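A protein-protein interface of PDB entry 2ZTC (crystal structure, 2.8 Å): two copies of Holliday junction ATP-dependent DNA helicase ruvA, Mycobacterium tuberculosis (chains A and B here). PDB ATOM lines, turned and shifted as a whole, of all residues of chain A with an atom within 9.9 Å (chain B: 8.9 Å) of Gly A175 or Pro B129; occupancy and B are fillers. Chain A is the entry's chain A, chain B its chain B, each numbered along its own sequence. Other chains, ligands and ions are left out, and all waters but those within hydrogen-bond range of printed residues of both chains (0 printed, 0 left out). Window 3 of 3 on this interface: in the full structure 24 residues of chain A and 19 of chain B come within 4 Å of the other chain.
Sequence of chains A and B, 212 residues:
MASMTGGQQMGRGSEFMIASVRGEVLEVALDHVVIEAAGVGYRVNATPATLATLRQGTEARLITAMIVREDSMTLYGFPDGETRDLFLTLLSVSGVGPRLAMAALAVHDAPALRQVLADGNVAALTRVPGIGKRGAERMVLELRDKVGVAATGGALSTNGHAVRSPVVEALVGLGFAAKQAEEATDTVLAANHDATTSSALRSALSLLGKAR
Of the 19 printed residues of chain B, 4 touch a printed residue of chain A. Printed residues of chain B that touch a printed residue of chain A: Ala B103, Ala B106, Arg B127 and Pro B129. Among the printed residues, 7 pairs touch across the chains. Among the printed residues, no Asp or Glu carboxylate lies within 4 Å of a Lys or Arg side-chain nitrogen of the other chain.
N of Phe A176 is in hydrogen-bond range of O of Leu A171 (3.4 Å).
The backbone carbonyl oxygen (O) of Gly A209 is in hydrogen-bond range of the guanidinium group (NH1) of Arg B127 (2.8 Å).
Among the printed residues, merely in contact across the chains: Gly A175 with Pro B129 (3.4 Å), Phe A176 with Pro B129 (3.5 Å), Leu A174 with Pro B129 (3.6 Å), Leu A205 with Ala B106 (3.7 Å), Leu A174 with Ala B106 (3.7 Å) and Leu A174 with Ala B103 (3.8 Å).
No position is printed for both chains.
Of chain B, only Pro B129 comes within 4 Å of Gly A175. Pro B129 touches three residues of chain A. No residue of chain B comes within 4 Å of Gly A173. Printed residues of chain B within 4 Å of Phe A176: Pro B129. No residue of chain A comes within 4 Å of Val B128. No residue of chain A comes within 4 Å of Gly B130. Of the printed residues of chain B, Leu A174 touches Ala B103 (3.8 Å), Ala B106 (3.7 Å) and Pro B129 (3.6 Å). Of the printed residues of chain A, Arg B127 touches Gly A209 (2.8 Å). Printed residues of chain A within 4 Å of Ala B103: Leu A174 (3.8 Å). Printed residues of chain B within 4 Å of Gly A209: Arg B127 (2.8 Å). Printed residues of chain A within 4 Å of Ala B106: Leu A174 (3.7 Å) and Leu A205 (3.7 Å). Leu A208 touches none of the printed residues of chain B. The nearest residue of chain A that does not touch Pro B129 is Leu A171 (5.9 Å). The nearest printed residue of chain A that does not touch Ala B106 is Phe A176 (7.3 Å).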
ATOM      1  N   GLY A  11      -8.230  10.730  10.746  1.00  0.00           N
ATOM      2  CA  GLY A  11      -7.795   9.620   9.906  1.00  0.00           C
ATOM      3  C   GLY A  11      -8.138   8.266  10.539  1.00  0.00           C
ATOM      4  O   GLY A  11      -7.645   7.228  10.094  1.00  0.00           O
ATOM      5  N   VAL A 167     -21.329  15.861  23.137  1.00  0.00           N
ATOM      6  CA  VAL A 167     -21.550  16.869  22.129  1.00  0.00           C
ATOM      7  C   VAL A 167     -20.274  17.352  21.499  1.00  0.00           C
ATOM      8  O   VAL A 167     -20.167  17.403  20.269  1.00  0.00           O
ATOM      9  CB  VAL A 167     -22.210  18.094  22.717  1.00  0.00           C
ATOM     10  CG1 VAL A 167     -22.217  19.180  21.678  1.00  0.00           C
ATOM     11  CG2 VAL A 167     -23.623  17.770  23.168  1.00  0.00           C
ATOM     12  N   VAL A 168     -19.318  17.760  22.327  1.00  0.00           N
ATOM     13  CA  VAL A 168     -18.129  18.363  21.754  1.00  0.00           C
ATOM     14  C   VAL A 168     -17.358  17.293  21.024  1.00  0.00           C
ATOM     15  O   VAL A 168     -16.671  17.564  20.036  1.00  0.00           O
ATOM     16  CB  VAL A 168     -17.220  19.012  22.788  1.00  0.00           C
ATOM     17  CG1 VAL A 168     -18.045  19.633  23.892  1.00  0.00           C
ATOM     18  CG2 VAL A 168     -16.235  18.007  23.301  1.00  0.00           C
ATOM     19  N   GLU A 169     -17.493  16.068  21.517  1.00  0.00           N
ATOM     20  CA  GLU A 169     -16.815  14.936  20.923  1.00  0.00           C
ATOM     21  C   GLU A 169     -17.237  14.868  19.456  1.00  0.00           C
ATOM     22  O   GLU A 169     -16.391  14.861  18.558  1.00  0.00           O
ATOM     23  CB  GLU A 169     -17.183  13.663  21.674  1.00  0.00           C
ATOM     24  CG  GLU A 169     -16.211  12.529  21.465  1.00  0.00           C
ATOM     25  CD  GLU A 169     -16.688  11.228  22.085  1.00  0.00           C
ATOM     26  OE1 GLU A 169     -17.874  10.880  21.903  1.00  0.00           O
ATOM     27  OE2 GLU A 169     -15.875  10.552  22.750  1.00  0.00           O
ATOM     28  N   ALA A 170     -18.554  14.860  19.237  1.00  0.00           N
ATOM     29  CA  ALA A 170     -19.149  14.868  17.903  1.00  0.00           C
ATOM     30  C   ALA A 170     -18.533  15.906  16.978  1.00  0.00           C
ATOM     31  O   ALA A 170     -18.147  15.591  15.853  1.00  0.00           O
ATOM     32  CB  ALA A 170     -20.657  15.089  17.993  1.00  0.00           C
ATOM     33  N   LEU A 171     -18.464  17.143  17.443  1.00  0.00           N
ATOM     34  CA  LEU A 171     -17.950  18.219  16.609  1.00  0.00           C
ATOM     35  C   LEU A 171     -16.531  17.888  16.225  1.00  0.00           C
ATOM     36  O   LEU A 171     -16.161  17.946  15.055  1.00  0.00           O
ATOM     37  CB  LEU A 171     -17.984  19.561  17.343  1.00  0.00           C
ATOM     38  CG  LEU A 171     -19.329  19.996  17.927  1.00  0.00           C
ATOM     39  CD1 LEU A 171     -19.162  21.214  18.835  1.00  0.00           C
ATOM     40  CD2 LEU A 171     -20.321  20.290  16.807  1.00  0.00           C
ATOM     41  N   VAL A 172     -15.729  17.537  17.217  1.00  0.00           N
ATOM     42  CA  VAL A 172     -14.342  17.211  16.945  1.00  0.00           C
ATOM     43  C   VAL A 172     -14.284  16.190  15.813  1.00  0.00           C
ATOM     44  O   VAL A 172     -13.360  16.180  14.990  1.00  0.00           O
ATOM     45  CB  VAL A 172     -13.664  16.651  18.180  1.00  0.00           C
ATOM     46  CG1 VAL A 172     -12.315  16.117  17.818  1.00  0.00           C
ATOM     47  CG2 VAL A 172     -13.531  17.741  19.231  1.00  0.00           C
ATOM     48  N   GLY A 173     -15.299  15.341  15.770  1.00  0.00           N
ATOM     49  CA  GLY A 173     -15.389  14.343  14.735  1.00  0.00           C
ATOM     50  C   GLY A 173     -15.692  14.952  13.391  1.00  0.00           C
ATOM     51  O   GLY A 173     -15.248  14.458  12.359  1.00  0.00           O
ATOM     52  N   LEU A 174     -16.468  16.027  13.408  1.00  0.00           N
ATOM     53  CA  LEU A 174     -16.791  16.743  12.182  1.00  0.00           C
ATOM     54  C   LEU A 174     -15.616  17.643  11.777  1.00  0.00           C
ATOM     55  O   LEU A 174     -15.727  18.448  10.861  1.00  0.00           O
ATOM     56  CB  LEU A 174     -18.102  17.526  12.336  1.00  0.00           C
ATOM     57  CG  LEU A 174     -19.425  16.750  12.520  1.00  0.00           C
ATOM     58  CD1 LEU A 174     -20.531  17.586  13.198  1.00  0.00           C
ATOM     59  CD2 LEU A 174     -19.957  16.199  11.200  1.00  0.00           C
ATOM     60  N   GLY A 175     -14.482  17.494  12.448  1.00  0.00           N
ATOM     61  CA  GLY A 175     -13.260  18.116  11.977  1.00  0.00           C
ATOM     62  C   GLY A 175     -12.847  19.365  12.720  1.00  0.00           C
ATOM     63  O   GLY A 175     -11.767  19.907  12.468  1.00  0.00           O
ATOM     64  N   PHE A 176     -13.706  19.825  13.626  1.00  0.00           N
ATOM     65  CA  PHE A 176     -13.393  20.967  14.481  1.00  0.00           C
ATOM     66  C   PHE A 176     -12.231  20.719  15.427  1.00  0.00           C
ATOM     67  O   PHE A 176     -11.646  19.634  15.456  1.00  0.00           O
ATOM     68  CB  PHE A 176     -14.592  21.318  15.331  1.00  0.00           C
ATOM     69  CG  PHE A 176     -15.699  21.936  14.570  1.00  0.00           C
ATOM     70  CD1 PHE A 176     -15.608  23.247  14.137  1.00  0.00           C
ATOM     71  CD2 PHE A 176     -16.840  21.217  14.284  1.00  0.00           C
ATOM     72  CE1 PHE A 176     -16.649  23.836  13.438  1.00  0.00           C
ATOM     73  CE2 PHE A 176     -17.875  21.796  13.583  1.00  0.00           C
ATOM     74  CZ  PHE A 176     -17.780  23.115  13.164  1.00  0.00           C
ATOM     75  N   ALA A 177     -11.928  21.735  16.229  1.00  0.00           N
ATOM     76  CA  ALA A 177     -10.829  21.663  17.173  1.00  0.00           C
ATOM     77  C   ALA A 177     -11.387  21.716  18.588  1.00  0.00           C
ATOM     78  O   ALA A 177     -12.367  22.423  18.842  1.00  0.00           O
ATOM     79  CB  ALA A 177      -9.863  22.814  16.938  1.00  0.00           C
ATOM     80  N   ALA A 178     -10.770  20.975  19.509  1.00  0.00           N
ATOM     81  CA  ALA A 178     -11.298  20.922  20.861  1.00  0.00           C
ATOM     82  C   ALA A 178     -11.640  22.334  21.400  1.00  0.00           C
ATOM     83  O   ALA A 178     -12.727  22.551  21.943  1.00  0.00           O
ATOM     84  CB  ALA A 178     -10.345  20.135  21.796  1.00  0.00           C
ATOM     85  N   LYS A 179     -10.745  23.302  21.211  1.00  0.00           N
ATOM     86  CA  LYS A 179     -11.038  24.683  21.614  1.00  0.00           C
ATOM     87  C   LYS A 179     -12.390  25.118  21.081  1.00  0.00           C
ATOM     88  O   LYS A 179     -13.317  25.339  21.843  1.00  0.00           O
ATOM     89  CB  LYS A 179      -9.956  25.652  21.133  1.00  0.00           C
ATOM     90  N   GLN A 180     -12.491  25.235  19.761  1.00  0.00           N
ATOM     91  CA  GLN A 180     -13.710  25.718  19.128  1.00  0.00           C
ATOM     92  C   GLN A 180     -14.937  24.917  19.560  1.00  0.00           C
ATOM     93  O   GLN A 180     -15.992  25.474  19.855  1.00  0.00           O
ATOM     94  CB  GLN A 180     -13.569  25.651  17.608  1.00  0.00           C
ATOM     95  CG  GLN A 180     -12.766  26.777  16.972  1.00  0.00           C
ATOM     96  CD  GLN A 180     -12.824  26.730  15.446  1.00  0.00           C
ATOM     97  OE1 GLN A 180     -13.416  27.605  14.809  1.00  0.00           O
ATOM     98  NE2 GLN A 180     -12.225  25.694  14.857  1.00  0.00           N
ATOM     99  N   ALA A 181     -14.791  23.600  19.581  1.00  0.00           N
ATOM    100  CA  ALA A 181     -15.900  22.713  19.888  1.00  0.00           C
ATOM    101  C   ALA A 181     -16.421  23.014  21.277  1.00  0.00           C
ATOM    102  O   ALA A 181     -17.608  23.264  21.440  1.00  0.00           O
ATOM    103  CB  ALA A 181     -15.461  21.261  19.774  1.00  0.00           C
ATOM    104  N   ALA A 204     -25.227  24.079  18.312  1.00  0.00           N
ATOM    105  CA  ALA A 204     -23.809  24.314  18.272  1.00  0.00           C
ATOM    106  C   ALA A 204     -23.344  24.387  16.806  1.00  0.00           C
ATOM    107  O   ALA A 204     -22.410  25.113  16.466  1.00  0.00           O
ATOM    108  CB  ALA A 204     -23.101  23.223  19.048  1.00  0.00           C
ATOM    109  N   LEU A 205     -24.012  23.654  15.928  1.00  0.00           N
ATOM    110  CA  LEU A 205     -23.654  23.730  14.522  1.00  0.00           C
ATOM    111  C   LEU A 205     -24.234  25.005  13.883  1.00  0.00           C
ATOM    112  O   LEU A 205     -23.522  25.731  13.179  1.00  0.00           O
ATOM    113  CB  LEU A 205     -24.022  22.431  13.787  1.00  0.00           C
ATOM    114  CG  LEU A 205     -23.238  21.172  14.262  1.00  0.00           C
ATOM    115  CD1 LEU A 205     -23.936  19.886  13.889  1.00  0.00           C
ATOM    116  CD2 LEU A 205     -21.809  21.099  13.760  1.00  0.00           C
ATOM    117  N   LEU A 208     -21.936  27.528  15.019  1.00  0.00           N
ATOM    118  CA  LEU A 208     -20.629  27.409  14.412  1.00  0.00           C
ATOM    119  C   LEU A 208     -20.604  27.779  12.937  1.00  0.00           C
ATOM    120  O   LEU A 208     -19.531  27.992  12.367  1.00  0.00           O
ATOM    121  CB  LEU A 208     -20.086  26.005  14.642  1.00  0.00           C
ATOM    122  CG  LEU A 208     -19.243  25.934  15.900  1.00  0.00           C
ATOM    123  CD1 LEU A 208     -19.270  24.535  16.430  1.00  0.00           C
ATOM    124  CD2 LEU A 208     -17.817  26.389  15.584  1.00  0.00           C
ATOM    125  N   GLY A 209     -21.784  27.861  12.328  1.00  0.00           N
ATOM    126  CA  GLY A 209     -21.887  28.246  10.930  1.00  0.00           C
ATOM    127  C   GLY A 209     -21.925  29.755  10.743  1.00  0.00           C
ATOM    128  O   GLY A 209     -22.210  30.234   9.636  1.00  0.00           O
ATOM    129  N   GLY B  97     -14.199  14.510   0.152  1.00  0.00           N
ATOM    130  CA  GLY B  97     -14.602  13.137   0.435  1.00  0.00           C
ATOM    131  C   GLY B  97     -15.865  13.059   1.277  1.00  0.00           C
ATOM    132  O   GLY B  97     -16.252  14.046   1.897  1.00  0.00           O
ATOM    133  N   ARG B  99     -16.691  12.054   4.241  1.00  0.00           N
ATOM    134  CA  ARG B  99     -16.666  12.655   5.552  1.00  0.00           C
ATOM    135  C   ARG B  99     -16.841  14.178   5.394  1.00  0.00           C
ATOM    136  O   ARG B  99     -17.686  14.784   6.046  1.00  0.00           O
ATOM    137  CB  ARG B  99     -15.425  12.281   6.341  1.00  0.00           C
ATOM    138  CG  ARG B  99     -15.581  10.961   7.075  1.00  0.00           C
ATOM    139  CD  ARG B  99     -14.479  10.776   8.097  1.00  0.00           C
ATOM    140  NE  ARG B  99     -13.193  10.541   7.452  1.00  0.00           N
ATOM    141  CZ  ARG B  99     -12.864   9.406   6.846  1.00  0.00           C
ATOM    142  NH1 ARG B  99     -13.727   8.401   6.813  1.00  0.00           N
ATOM    143  NH2 ARG B  99     -11.672   9.274   6.279  1.00  0.00           N
ATOM    144  N   LEU B 100     -16.025  14.775   4.532  1.00  0.00           N
ATOM    145  CA  LEU B 100     -16.063  16.223   4.319  1.00  0.00           C
ATOM    146  C   LEU B 100     -17.460  16.665   3.973  1.00  0.00           C
ATOM    147  O   LEU B 100     -18.019  17.544   4.627  1.00  0.00           O
ATOM    148  CB  LEU B 100     -15.142  16.621   3.171  1.00  0.00           C
ATOM    149  CG  LEU B 100     -15.143  18.097   2.799  1.00  0.00           C
ATOM    150  CD1 LEU B 100     -14.639  18.927   3.962  1.00  0.00           C
ATOM    151  CD2 LEU B 100     -14.271  18.310   1.567  1.00  0.00           C
ATOM    152  N   ALA B 101     -18.010  16.060   2.923  1.00  0.00           N
ATOM    153  CA  ALA B 101     -19.349  16.392   2.439  1.00  0.00           C
ATOM    154  C   ALA B 101     -20.380  16.336   3.565  1.00  0.00           C
ATOM    155  O   ALA B 101     -21.250  17.207   3.680  1.00  0.00           O
ATOM    156  CB  ALA B 101     -19.738  15.452   1.339  1.00  0.00           C
ATOM    157  N   MET B 102     -20.276  15.303   4.397  1.00  0.00           N
ATOM    158  CA  MET B 102     -21.179  15.156   5.527  1.00  0.00           C
ATOM    159  C   MET B 102     -20.989  16.302   6.516  1.00  0.00           C
ATOM    160  O   MET B 102     -21.965  16.860   7.017  1.00  0.00           O
ATOM    161  CB  MET B 102     -20.992  13.793   6.196  1.00  0.00           C
ATOM    162  CG  MET B 102     -21.601  12.656   5.387  1.00  0.00           C
ATOM    163  SD  MET B 102     -23.409  12.798   5.334  1.00  0.00           S
ATOM    164  CE  MET B 102     -23.796  12.397   7.040  1.00  0.00           C
ATOM    165  N   ALA B 103     -19.734  16.671   6.765  1.00  0.00           N
ATOM    166  CA  ALA B 103     -19.429  17.785   7.659  1.00  0.00           C
ATOM    167  C   ALA B 103     -20.140  19.055   7.179  1.00  0.00           C
ATOM    168  O   ALA B 103     -20.814  19.737   7.962  1.00  0.00           O
ATOM    169  CB  ALA B 103     -17.917  18.002   7.775  1.00  0.00           C
ATOM    170  N   ALA B 104     -20.013  19.356   5.887  1.00  0.00           N
ATOM    171  CA  ALA B 104     -20.649  20.557   5.341  1.00  0.00           C
ATOM    172  C   ALA B 104     -22.158  20.531   5.558  1.00  0.00           C
ATOM    173  O   ALA B 104     -22.730  21.494   6.046  1.00  0.00           O
ATOM    174  CB  ALA B 104     -20.322  20.710   3.895  1.00  0.00           C
ATOM    175  N   ALA B 106     -23.711  18.934   7.716  1.00  0.00           N
ATOM    176  CA  ALA B 106     -24.001  18.840   9.118  1.00  0.00           C
ATOM    177  C   ALA B 106     -24.110  20.261   9.617  1.00  0.00           C
ATOM    178  O   ALA B 106     -24.966  20.591  10.451  1.00  0.00           O
ATOM    179  CB  ALA B 106     -22.884  18.092   9.823  1.00  0.00           C
ATOM    180  N   VAL B 107     -23.243  21.098   9.062  1.00  0.00           N
ATOM    181  CA  VAL B 107     -23.190  22.509   9.393  1.00  0.00           C
ATOM    182  C   VAL B 107     -24.300  23.294   8.696  1.00  0.00           C
ATOM    183  O   VAL B 107     -24.996  24.108   9.314  1.00  0.00           O
ATOM    184  CB  VAL B 107     -21.847  23.098   8.964  1.00  0.00           C
ATOM    185  CG1 VAL B 107     -21.802  24.576   9.297  1.00  0.00           C
ATOM    186  CG2 VAL B 107     -20.692  22.332   9.622  1.00  0.00           C
ATOM    187  N   HIS B 108     -24.451  23.050   7.401  1.00  0.00           N
ATOM    188  CA  HIS B 108     -25.441  23.747   6.587  1.00  0.00           C
ATOM    189  C   HIS B 108     -26.432  22.759   5.970  1.00  0.00           C
ATOM    190  O   HIS B 108     -26.065  21.952   5.096  1.00  0.00           O
ATOM    191  CB  HIS B 108     -24.762  24.500   5.431  1.00  0.00           C
ATOM    192  CG  HIS B 108     -23.757  25.527   5.863  1.00  0.00           C
ATOM    193  ND1 HIS B 108     -24.103  26.643   6.583  1.00  0.00           N
ATOM    194  CD2 HIS B 108     -22.426  25.613   5.631  1.00  0.00           C
ATOM    195  CE1 HIS B 108     -23.015  27.371   6.801  1.00  0.00           C
ATOM    196  NE2 HIS B 108     -21.991  26.769   6.234  1.00  0.00           N
ATOM    197  N   ALA B 124     -19.096  31.511   4.398  1.00  0.00           N
ATOM    198  CA  ALA B 124     -19.915  30.461   4.987  1.00  0.00           C
ATOM    199  C   ALA B 124     -19.255  29.073   4.872  1.00  0.00           C
ATOM    200  O   ALA B 124     -19.307  28.270   5.806  1.00  0.00           O
ATOM    201  CB  ALA B 124     -21.295  30.461   4.348  1.00  0.00           C
ATOM    202  N   LEU B 125     -18.637  28.811   3.720  1.00  0.00           N
ATOM    203  CA  LEU B 125     -17.999  27.530   3.453  1.00  0.00           C
ATOM    204  C   LEU B 125     -16.740  27.313   4.278  1.00  0.00           C
ATOM    205  O   LEU B 125     -16.475  26.203   4.725  1.00  0.00           O
ATOM    206  CB  LEU B 125     -17.648  27.401   1.967  1.00  0.00           C
ATOM    207  CG  LEU B 125     -18.810  27.362   0.972  1.00  0.00           C
ATOM    208  CD1 LEU B 125     -18.293  27.159  -0.452  1.00  0.00           C
ATOM    209  CD2 LEU B 125     -19.806  26.271   1.338  1.00  0.00           C
ATOM    210  N   THR B 126     -15.955  28.365   4.462  1.00  0.00           N
ATOM    211  CA  THR B 126     -14.710  28.245   5.196  1.00  0.00           C
ATOM    212  C   THR B 126     -15.028  27.931   6.653  1.00  0.00           C
ATOM    213  O   THR B 126     -14.219  27.350   7.383  1.00  0.00           O
ATOM    214  CB  THR B 126     -13.883  29.524   5.110  1.00  0.00           C
ATOM    215  OG1 THR B 126     -13.559  29.783   3.741  1.00  0.00           O
ATOM    216  CG2 THR B 126     -12.595  29.373   5.910  1.00  0.00           C
ATOM    217  N   ARG B 127     -16.234  28.300   7.058  1.00  0.00           N
ATOM    218  CA  ARG B 127     -16.728  28.000   8.395  1.00  0.00           C
ATOM    219  C   ARG B 127     -16.786  26.480   8.632  1.00  0.00           C
ATOM    220  O   ARG B 127     -17.012  26.027   9.753  1.00  0.00           O
ATOM    221  CB  ARG B 127     -18.097  28.676   8.646  1.00  0.00           C
ATOM    222  CG  ARG B 127     -18.074  30.202   8.510  1.00  0.00           C
ATOM    223  CD  ARG B 127     -19.311  30.890   9.101  1.00  0.00           C
ATOM    224  NE  ARG B 127     -19.427  32.273   8.631  1.00  0.00           N
ATOM    225  CZ  ARG B 127     -20.443  32.741   7.908  1.00  0.00           C
ATOM    226  NH1 ARG B 127     -21.464  31.954   7.592  1.00  0.00           N
ATOM    227  NH2 ARG B 127     -20.454  34.007   7.510  1.00  0.00           N
ATOM    228  N   VAL B 128     -16.551  25.701   7.579  1.00  0.00           N
ATOM    229  CA  VAL B 128     -16.605  24.234   7.654  1.00  0.00           C
ATOM    230  C   VAL B 128     -15.208  23.611   7.669  1.00  0.00           C
ATOM    231  O   VAL B 128     -14.435  23.790   6.721  1.00  0.00           O
ATOM    232  CB  VAL B 128     -17.446  23.645   6.493  1.00  0.00           C
ATOM    233  CG1 VAL B 128     -17.272  22.147   6.398  1.00  0.00           C
ATOM    234  CG2 VAL B 128     -18.911  23.989   6.685  1.00  0.00           C
ATOM    235  N   PRO B 129     -14.887  22.879   8.755  1.00  0.00           N
ATOM    236  CA  PRO B 129     -13.571  22.296   9.021  1.00  0.00           C
ATOM    237  C   PRO B 129     -13.086  21.446   7.862  1.00  0.00           C
ATOM    238  O   PRO B 129     -13.807  20.562   7.406  1.00  0.00           O
ATOM    239  CB  PRO B 129     -13.824  21.394  10.230  1.00  0.00           C
ATOM    240  CG  PRO B 129     -14.982  21.977  10.908  1.00  0.00           C
ATOM    241  CD  PRO B 129     -15.843  22.578   9.834  1.00  0.00           C
ATOM    242  N   GLY B 130     -11.864  21.698   7.409  1.00  0.00           N
ATOM    243  CA  GLY B 130     -11.284  20.948   6.311  1.00  0.00           C
ATOM    244  C   GLY B 130     -11.308  21.745   5.019  1.00  0.00           C
ATOM    245  O   GLY B 130     -10.545  21.483   4.091  1.00  0.00           O
ATOM    246  N   ILE B 131     -12.189  22.732   4.966  1.00  0.00           N
ATOM    247  CA  ILE B 131     -12.333  23.569   3.789  1.00  0.00           C
ATOM    248  C   ILE B 131     -11.504  24.841   3.918  1.00  0.00           C
ATOM    249  O   ILE B 131     -11.825  25.727   4.731  1.00  0.00           O
ATOM    250  CB  ILE B 131     -13.802  23.930   3.575  1.00  0.00           C
ATOM    251  CG1 ILE B 131     -14.597  22.671   3.219  1.00  0.00           C
ATOM    252  CG2 ILE B 131     -13.949  24.982   2.491  1.00  0.00           C
ATOM    253  CD1 ILE B 131     -16.069  22.941   3.005  1.00  0.00           C
ATOM    254  N   GLY B 132     -10.440  24.911   3.116  1.00  0.00           N
ATOM    255  CA  GLY B 132      -9.553  26.062   3.078  1.00  0.00           C
ATOM    256  C   GLY B 132     -10.120  27.155   2.198  1.00  0.00           C
ATOM    257  O   GLY B 132     -11.068  26.921   1.451  1.00  0.00           O
